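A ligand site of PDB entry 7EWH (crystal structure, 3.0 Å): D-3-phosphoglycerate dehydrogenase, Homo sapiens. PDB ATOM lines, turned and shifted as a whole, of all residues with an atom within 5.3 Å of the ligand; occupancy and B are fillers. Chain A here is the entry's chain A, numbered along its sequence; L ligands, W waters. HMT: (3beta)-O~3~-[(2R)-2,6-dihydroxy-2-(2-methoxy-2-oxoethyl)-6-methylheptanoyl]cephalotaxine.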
ATOM      1  N   THR A  73      27.139  32.633  11.009  1.00  0.00           N
ATOM      2  CA  THR A  73      27.459  31.220  10.821  1.00  0.00           C
ATOM      3  C   THR A  73      28.755  31.046  10.050  1.00  0.00           C
ATOM      4  O   THR A  73      28.985  31.687   9.025  1.00  0.00           O
ATOM      5  CB  THR A  73      26.336  30.504  10.064  1.00  0.00           C
ATOM      6  OG1 THR A  73      26.196  31.045   8.739  1.00  0.00           O
ATOM      7  CG2 THR A  73      25.026  30.641  10.806  1.00  0.00           C
ATOM      8  N   PRO A  94      27.865  30.731  16.286  1.00  0.00           N
ATOM      9  CA  PRO A  94      27.109  29.611  15.718  1.00  0.00           C
ATOM     10  C   PRO A  94      25.648  29.572  16.125  1.00  0.00           C
ATOM     11  O   PRO A  94      24.883  28.784  15.528  1.00  0.00           O
ATOM     12  CB  PRO A  94      27.856  28.395  16.275  1.00  0.00           C
ATOM     13  CG  PRO A  94      28.310  28.870  17.627  1.00  0.00           C
ATOM     14  CD  PRO A  94      28.589  30.354  17.507  1.00  0.00           C
ATOM     15  N   SER A  98      20.638  30.660  13.574  1.00  0.00           N
ATOM     16  CA  SER A  98      19.865  29.445  13.405  1.00  0.00           C
ATOM     17  C   SER A  98      18.390  29.719  13.183  1.00  0.00           C
ATOM     18  O   SER A  98      17.762  29.157  12.274  1.00  0.00           O
ATOM     19  CB  SER A  98      20.078  28.560  14.609  1.00  0.00           C
ATOM     20  OG  SER A  98      21.436  28.653  14.986  1.00  0.00           O
ATOM     21  N   ILE A 145      15.633  17.127   4.515  1.00  0.00           N
ATOM     22  CA  ILE A 145      16.535  18.081   5.168  1.00  0.00           C
ATOM     23  C   ILE A 145      17.863  17.361   5.356  1.00  0.00           C
ATOM     24  O   ILE A 145      18.010  16.518   6.246  1.00  0.00           O
ATOM     25  CB  ILE A 145      15.978  18.588   6.497  1.00  0.00           C
ATOM     26  CG1 ILE A 145      14.519  18.979   6.332  1.00  0.00           C
ATOM     27  CG2 ILE A 145      16.733  19.788   7.000  1.00  0.00           C
ATOM     28  CD1 ILE A 145      13.543  17.872   6.708  1.00  0.00           C
ATOM     29  N   LEU A 146      18.853  17.738   4.543  1.00  0.00           N
ATOM     30  CA  LEU A 146      20.137  17.054   4.511  1.00  0.00           C
ATOM     31  C   LEU A 146      21.014  17.677   5.581  1.00  0.00           C
ATOM     32  O   LEU A 146      21.266  18.883   5.543  1.00  0.00           O
ATOM     33  CB  LEU A 146      20.766  17.175   3.118  1.00  0.00           C
ATOM     34  CG  LEU A 146      20.105  16.458   1.927  1.00  0.00           C
ATOM     35  CD1 LEU A 146      21.107  16.131   0.859  1.00  0.00           C
ATOM     36  CD2 LEU A 146      19.406  15.192   2.346  1.00  0.00           C
ATOM     37  N   GLY A 147      21.462  16.863   6.537  1.00  0.00           N
ATOM     38  CA  GLY A 147      22.130  17.471   7.664  1.00  0.00           C
ATOM     39  C   GLY A 147      21.102  18.089   8.599  1.00  0.00           C
ATOM     40  O   GLY A 147      20.205  18.807   8.150  1.00  0.00           O
ATOM     41  N   LEU A 148      21.196  17.806   9.876  1.00  0.00           N
ATOM     42  CA  LEU A 148      20.257  18.356  10.813  1.00  0.00           C
ATOM     43  C   LEU A 148      21.079  19.243  11.743  1.00  0.00           C
ATOM     44  O   LEU A 148      22.237  19.560  11.451  1.00  0.00           O
ATOM     45  CB  LEU A 148      19.497  17.248  11.540  1.00  0.00           C
ATOM     46  CG  LEU A 148      18.549  16.220  10.899  1.00  0.00           C
ATOM     47  CD1 LEU A 148      17.575  16.839   9.982  1.00  0.00           C
ATOM     48  CD2 LEU A 148      19.207  15.060  10.222  1.00  0.00           C
ATOM     49  N   GLY A 149      20.481  19.664  12.846  1.00  0.00           N
ATOM     50  CA  GLY A 149      21.210  20.503  13.770  1.00  0.00           C
ATOM     51  C   GLY A 149      20.376  21.692  14.166  1.00  0.00           C
ATOM     52  O   GLY A 149      19.148  21.565  14.260  1.00  0.00           O
ATOM     53  N   ARG A 150      20.978  22.869  14.327  1.00  0.00           N
ATOM     54  CA  ARG A 150      20.199  24.055  14.633  1.00  0.00           C
ATOM     55  C   ARG A 150      19.144  24.312  13.560  1.00  0.00           C
ATOM     56  O   ARG A 150      17.935  24.097  13.790  1.00  0.00           O
ATOM     57  CB  ARG A 150      21.120  25.274  14.801  1.00  0.00           C
ATOM     58  CG  ARG A 150      22.004  25.296  16.068  1.00  0.00           C
ATOM     59  CD  ARG A 150      23.472  24.952  15.824  1.00  0.00           C
ATOM     60  NE  ARG A 150      24.374  25.666  16.742  1.00  0.00           N
ATOM     61  CZ  ARG A 150      25.517  25.168  17.223  1.00  0.00           C
ATOM     62  NH1 ARG A 150      25.920  23.943  16.897  1.00  0.00           N
ATOM     63  NH2 ARG A 150      26.254  25.905  18.054  1.00  0.00           N
ATOM     64  N   ILE A 151      19.588  24.766  12.383  1.00  0.00           N
ATOM     65  CA  ILE A 151      18.665  25.216  11.340  1.00  0.00           C
ATOM     66  C   ILE A 151      17.805  24.066  10.852  1.00  0.00           C
ATOM     67  O   ILE A 151      16.621  24.238  10.574  1.00  0.00           O
ATOM     68  CB  ILE A 151      19.413  25.890  10.189  1.00  0.00           C
ATOM     69  CG1 ILE A 151      20.072  27.170  10.663  1.00  0.00           C
ATOM     70  CG2 ILE A 151      18.448  26.240   9.081  1.00  0.00           C
ATOM     71  CD1 ILE A 151      20.776  27.878   9.558  1.00  0.00           C
ATOM     72  N   GLY A 152      18.400  22.890  10.681  1.00  0.00           N
ATOM     73  CA  GLY A 152      17.643  21.779  10.136  1.00  0.00           C
ATOM     74  C   GLY A 152      16.492  21.333  11.016  1.00  0.00           C
ATOM     75  O   GLY A 152      15.378  21.128  10.536  1.00  0.00           O
ATOM     76  N   ARG A 153      16.745  21.171  12.318  1.00  0.00           N
ATOM     77  CA  ARG A 153      15.671  20.794  13.238  1.00  0.00           C
ATOM     78  C   ARG A 153      14.627  21.900  13.409  1.00  0.00           C
ATOM     79  O   ARG A 153      13.444  21.599  13.631  1.00  0.00           O
ATOM     80  CB  ARG A 153      16.239  20.396  14.600  1.00  0.00           C
ATOM     81  CG  ARG A 153      16.213  21.511  15.622  1.00  0.00           C
ATOM     82  CD  ARG A 153      16.666  21.045  16.972  1.00  0.00           C
ATOM     83  NE  ARG A 153      18.112  21.157  17.155  1.00  0.00           N
ATOM     84  CZ  ARG A 153      18.981  20.159  17.008  1.00  0.00           C
ATOM     85  NH1 ARG A 153      18.544  18.960  16.668  1.00  0.00           N
ATOM     86  NH2 ARG A 153      20.274  20.361  17.191  1.00  0.00           N
ATOM     87  N   TYR A 169      19.025  13.559   6.601  1.00  0.00           N
ATOM     88  CA  TYR A 169      20.193  12.720   6.917  1.00  0.00           C
ATOM     89  C   TYR A 169      21.344  13.548   7.495  1.00  0.00           C
ATOM     90  O   TYR A 169      21.916  14.410   6.816  1.00  0.00           O
ATOM     91  CB  TYR A 169      20.647  11.976   5.653  1.00  0.00           C
ATOM     92  CG  TYR A 169      22.012  11.350   5.740  1.00  0.00           C
ATOM     93  CD1 TYR A 169      22.371  10.495   6.764  1.00  0.00           C
ATOM     94  CD2 TYR A 169      22.971  11.639   4.773  1.00  0.00           C
ATOM     95  CE1 TYR A 169      23.640   9.925   6.806  1.00  0.00           C
ATOM     96  CE2 TYR A 169      24.227  11.083   4.818  1.00  0.00           C
ATOM     97  CZ  TYR A 169      24.552  10.240   5.822  1.00  0.00           C
ATOM     98  OH  TYR A 169      25.824   9.721   5.825  1.00  0.00           O
ATOM     99  N   ASP A 170      21.700  13.242   8.751  1.00  0.00           N
ATOM    100  CA  ASP A 170      22.915  13.759   9.388  1.00  0.00           C
ATOM    101  C   ASP A 170      23.626  12.546   9.964  1.00  0.00           C
ATOM    102  O   ASP A 170      23.036  11.798  10.781  1.00  0.00           O
ATOM    103  CB  ASP A 170      22.607  14.787  10.467  1.00  0.00           C
ATOM    104  CG  ASP A 170      23.759  15.756  10.697  1.00  0.00           C
ATOM    105  OD1 ASP A 170      24.906  15.286  10.693  1.00  0.00           O
ATOM    106  OD2 ASP A 170      23.518  16.967  10.876  1.00  0.00           O
ATOM    107  N   PRO A 171      24.871  12.301   9.585  1.00  0.00           N
ATOM    108  CA  PRO A 171      25.568  11.080  10.035  1.00  0.00           C
ATOM    109  C   PRO A 171      25.801  11.093  11.529  1.00  0.00           C
ATOM    110  O   PRO A 171      25.458  10.153  12.246  1.00  0.00           O
ATOM    111  CB  PRO A 171      26.878  11.105   9.247  1.00  0.00           C
ATOM    112  CG  PRO A 171      27.083  12.565   8.913  1.00  0.00           C
ATOM    113  CD  PRO A 171      25.716  13.136   8.711  1.00  0.00           C
ATOM    114  N   ILE A 172      26.363  12.207  12.011  1.00  0.00           N
ATOM    115  CA  ILE A 172      26.603  12.335  13.448  1.00  0.00           C
ATOM    116  C   ILE A 172      25.291  12.213  14.215  1.00  0.00           C
ATOM    117  O   ILE A 172      25.167  11.409  15.149  1.00  0.00           O
ATOM    118  CB  ILE A 172      27.345  13.667  13.744  1.00  0.00           C
ATOM    119  CG1 ILE A 172      26.512  14.902  13.339  1.00  0.00           C
ATOM    120  CG2 ILE A 172      28.693  13.688  13.039  1.00  0.00           C
ATOM    121  CD1 ILE A 172      26.792  16.152  14.153  1.00  0.00           C
ATOM    122  N   ILE A 173      24.267  12.970  13.797  1.00  0.00           N
ATOM    123  CA  ILE A 173      23.067  13.132  14.613  1.00  0.00           C
ATOM    124  C   ILE A 173      22.375  11.795  14.730  1.00  0.00           C
ATOM    125  O   ILE A 173      22.165  11.094  13.723  1.00  0.00           O
ATOM    126  CB  ILE A 173      22.155  14.209  14.015  1.00  0.00           C
ATOM    127  CG1 ILE A 173      22.916  15.536  13.941  1.00  0.00           C
ATOM    128  CG2 ILE A 173      20.835  14.253  14.757  1.00  0.00           C
ATOM    129  CD1 ILE A 173      22.931  16.331  15.194  1.00  0.00           C
ATOM    130  N   THR A 199      15.743  20.607   1.532  1.00  0.00           N
ATOM    131  CA  THR A 199      16.430  21.761   2.082  1.00  0.00           C
ATOM    132  C   THR A 199      17.850  21.365   2.469  1.00  0.00           C
ATOM    133  O   THR A 199      18.108  20.214   2.806  1.00  0.00           O
ATOM    134  CB  THR A 199      15.709  22.295   3.305  1.00  0.00           C
ATOM    135  OG1 THR A 199      14.413  22.834   2.946  1.00  0.00           O
ATOM    136  CG2 THR A 199      16.528  23.358   3.997  1.00  0.00           C
ATOM    137  N   VAL A 200      18.761  22.341   2.430  1.00  0.00           N
ATOM    138  CA  VAL A 200      20.149  22.147   2.859  1.00  0.00           C
ATOM    139  C   VAL A 200      20.608  23.326   3.709  1.00  0.00           C
ATOM    140  O   VAL A 200      20.263  24.481   3.429  1.00  0.00           O
ATOM    141  CB  VAL A 200      21.086  22.003   1.653  1.00  0.00           C
ATOM    142  CG1 VAL A 200      22.523  21.837   2.112  1.00  0.00           C
ATOM    143  CG2 VAL A 200      20.639  20.861   0.730  1.00  0.00           C
ATOM    144  N   HIS A 201      21.401  23.015   4.755  1.00  0.00           N
ATOM    145  CA  HIS A 201      22.180  24.004   5.489  1.00  0.00           C
ATOM    146  C   HIS A 201      23.503  23.415   5.972  1.00  0.00           C
ATOM    147  O   HIS A 201      24.253  24.115   6.673  1.00  0.00           O
ATOM    148  CB  HIS A 201      21.398  24.581   6.687  1.00  0.00           C
ATOM    149  CG  HIS A 201      20.182  25.344   6.290  1.00  0.00           C
ATOM    150  ND1 HIS A 201      19.005  24.722   5.930  1.00  0.00           N
ATOM    151  CD2 HIS A 201      19.946  26.677   6.179  1.00  0.00           C
ATOM    152  CE1 HIS A 201      18.093  25.640   5.626  1.00  0.00           C
ATOM    153  NE2 HIS A 201      18.647  26.830   5.766  1.00  0.00           N
ATOM    154  N   THR A 202      23.800  22.143   5.639  1.00  0.00           N
ATOM    155  CA  THR A 202      25.069  21.424   5.731  1.00  0.00           C
ATOM    156  C   THR A 202      26.251  22.347   5.481  1.00  0.00           C
ATOM    157  O   THR A 202      26.234  23.156   4.539  1.00  0.00           O
ATOM    158  CB  THR A 202      25.056  20.265   4.748  1.00  0.00           C
ATOM    159  OG1 THR A 202      24.306  19.193   5.309  1.00  0.00           O
ATOM    160  CG2 THR A 202      26.431  19.808   4.463  1.00  0.00           C
ATOM    161  N   PRO A 203      27.312  22.239   6.269  1.00  0.00           N
ATOM    162  CA  PRO A 203      28.484  23.080   6.031  1.00  0.00           C
ATOM    163  C   PRO A 203      29.194  22.745   4.728  1.00  0.00           C
ATOM    164  O   PRO A 203      29.029  21.685   4.127  1.00  0.00           O
ATOM    165  CB  PRO A 203      29.374  22.768   7.236  1.00  0.00           C
ATOM    166  CG  PRO A 203      28.984  21.370   7.634  1.00  0.00           C
ATOM    167  CD  PRO A 203      27.544  21.218   7.300  1.00  0.00           C
ATOM    168  N   SER A 207      33.686  16.807   1.857  1.00  0.00           N
ATOM    169  CA  SER A 207      32.618  15.894   2.219  1.00  0.00           C
ATOM    170  C   SER A 207      31.306  16.326   1.559  1.00  0.00           C
ATOM    171  O   SER A 207      30.523  15.480   1.132  1.00  0.00           O
ATOM    172  CB  SER A 207      32.501  15.869   3.755  1.00  0.00           C
ATOM    173  OG  SER A 207      31.355  15.192   4.267  1.00  0.00           O
ATOM    174  N   THR A 208      31.086  17.639   1.403  1.00  0.00           N
ATOM    175  CA  THR A 208      29.803  18.128   0.911  1.00  0.00           C
ATOM    176  C   THR A 208      29.859  19.141  -0.238  1.00  0.00           C
ATOM    177  O   THR A 208      28.793  19.546  -0.735  1.00  0.00           O
ATOM    178  CB  THR A 208      28.997  18.746   2.055  1.00  0.00           C
ATOM    179  OG1 THR A 208      29.641  19.946   2.500  1.00  0.00           O
ATOM    180  CG2 THR A 208      28.885  17.779   3.200  1.00  0.00           C
HETATM  181  C18 HMT L   1      24.513  21.643  14.678  1.00  0.00           C
HETATM  182  O3  HMT L   1      25.715  22.283  14.295  1.00  0.00           O
HETATM  183  C2  HMT L   1      25.758  22.802  12.986  1.00  0.00           C
HETATM  184  C1  HMT L   1      26.047  24.232  12.650  1.00  0.00           C
HETATM  185  C9  HMT L   1      25.353  24.569  11.350  1.00  0.00           C
HETATM  186  C12 HMT L   1      26.304  24.961  10.210  1.00  0.00           C
HETATM  187  C11 HMT L   1      25.606  25.952   9.258  1.00  0.00           C
HETATM  188  C10 HMT L   1      24.138  26.010   9.717  1.00  0.00           C
HETATM  189  N1  HMT L   1      24.196  25.475  11.121  1.00  0.00           N
HETATM  190  C8  HMT L   1      23.149  25.325  12.092  1.00  0.00           C
HETATM  191  C7  HMT L   1      22.827  23.854  12.222  1.00  0.00           C
HETATM  192  C6  HMT L   1      22.733  23.136  10.890  1.00  0.00           C
HETATM  193  C16 HMT L   1      21.325  22.753  10.353  1.00  0.00           C
HETATM  194  C15 HMT L   1      21.204  22.000   8.981  1.00  0.00           C
HETATM  195  O2  HMT L   1      20.060  21.542   8.238  1.00  0.00           O
HETATM  196  C17 HMT L   1      20.523  21.326   6.978  1.00  0.00           C
HETATM  197  O1  HMT L   1      22.044  21.042   7.109  1.00  0.00           O
HETATM  198  C14 HMT L   1      22.424  21.643   8.196  1.00  0.00           C
HETATM  199  C13 HMT L   1      23.837  22.039   8.767  1.00  0.00           C
HETATM  200  C5  HMT L   1      23.952  22.773  10.124  1.00  0.00           C
HETATM  201  C4  HMT L   1      25.317  23.144  10.656  1.00  0.00           C
HETATM  202  C3  HMT L   1      25.725  22.041  11.679  1.00  0.00           C
HETATM  203  O4  HMT L   1      24.823  20.953  11.602  1.00  0.00           O
HETATM  204  C19 HMT L   1      25.301  19.571  11.389  1.00  0.00           C
HETATM  205  O5  HMT L   1      25.112  18.698  12.181  1.00  0.00           O
HETATM  206  C20 HMT L   1      26.079  19.209  10.136  1.00  0.00           C
HETATM  207  C21 HMT L   1      26.280  17.723   9.863  1.00  0.00           C
HETATM  208  C22 HMT L   1      26.039  17.425   8.347  1.00  0.00           C
HETATM  209  O8  HMT L   1      25.181  18.018   7.770  1.00  0.00           O
HETATM  210  O7  HMT L   1      26.810  16.435   7.643  1.00  0.00           O
HETATM  211  C23 HMT L   1      27.207  16.672   6.303  1.00  0.00           C
HETATM  212  O6  HMT L   1      25.344  19.748   9.072  1.00  0.00           O
HETATM  213  C24 HMT L   1      27.489  19.789  10.336  1.00  0.00           C
HETATM  214  C25 HMT L   1      28.146  19.065  11.560  1.00  0.00           C
HETATM  215  C26 HMT L   1      28.200  19.979  12.830  1.00  0.00           C
HETATM  216  C27 HMT L   1      29.555  20.762  12.836  1.00  0.00           C
HETATM  217  C28 HMT L   1      29.346  22.122  12.107  1.00  0.00           C
HETATM  218  C29 HMT L   1      30.001  20.968  14.323  1.00  0.00           C
HETATM  219  O9  HMT L   1      30.525  20.007  12.134  1.00  0.00           O
HETATM  220  O   HOH W   1      24.381  15.598   6.464  1.00  0.00           O
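N of Thr 202 lies within hydrogen-bond range of O1 of the ligand (2.5 Å).
OG1 of Thr 202 is in hydrogen-bond range of O8 of the ligand, 2.9 Å away.
The side-chain carboxylate (OD2) of Asp 170 sits close to an oxygen (O5) of the ligand, at 2.7 Å.
An oxygen (O2) of the ligand sits close to the backbone carbonyl oxygen (O) of Gly 147.
The backbone NH of His 201 sits close to an oxygen (O1) of the ligand.
The backbone NH (N) of Gly 152 lies close to an oxygen (O2) of the ligand (3.2 Å).
The guanidinium group (NH1) of Arg 150 sits at hydrogen-bond distance from an oxygen (O3) of the ligand, 3.1 Å away.
OG1 of Thr 202 sits at hydrogen-bond distance from O of Leu 146 (3.1 Å).
The side-chain carboxylate of Asp 170 sits at hydrogen-bond distance from the backbone NH of Leu 148 (2.7 Å).
O of Tyr 169 is in hydrogen-bond range of N of Gly 147 (2.5 Å).
N of Leu 146 sits at hydrogen-bond distance from O of Thr 199, at 3.1 Å.
The guanidinium group (NE) of Arg 150 sits at hydrogen-bond distance from the backbone carbonyl oxygen (O) of Pro 94 (3.4 Å).
OG1 of Thr 208 is in hydrogen-bond range of O of Pro 203 (2.5 Å).
NE of Arg 153 lies close to O of Gly 149 (3.1 Å).
The backbone NH (N) of Tyr 169 sits at hydrogen-bond distance from the backbone carbonyl oxygen (O) of Ile 145 (3.1 Å).
O of Leu 146 lies close to O1 of the ligand.
The backbone carbonyl oxygen of Leu 148 lies close to an oxygen (O4) of the ligand, at 2.9 Å.
Residues that only touch the ligand: Pro 203 (3.2 Å), Ile 151 (3.3 Å), Gly 149 (3.6 Å), Ile 172 (3.6 Å), Pro 171 (3.6 Å), Thr 208 (3.7 Å), Val 200 (3.8 Å) and Ile 145 (3.96 Å).
Hydrophobic or aromatic side chains within 4 Å of the ligand: Ile 145, Ile 151, Pro 171, Ile 172, His 201 and Pro 203.
16 residues have an atom within 4 Å of the ligand: Ile 145, Leu 146, Gly 147, Leu 148, Gly 149, Arg 150, Ile 151, Gly 152, Asp 170, Pro 171, Ile 172, Val 200, His 201, Thr 202, Pro 203 and Thr 208.
The nearest printed residue that does not touch the ligand is Ile 173 (4.2 Å).
Water W1 lies within hydrogen-bond range of the backbone carbonyl oxygen of Tyr 169, an oxygen (O7) of the ligand and the backbone NH of Gly 147.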
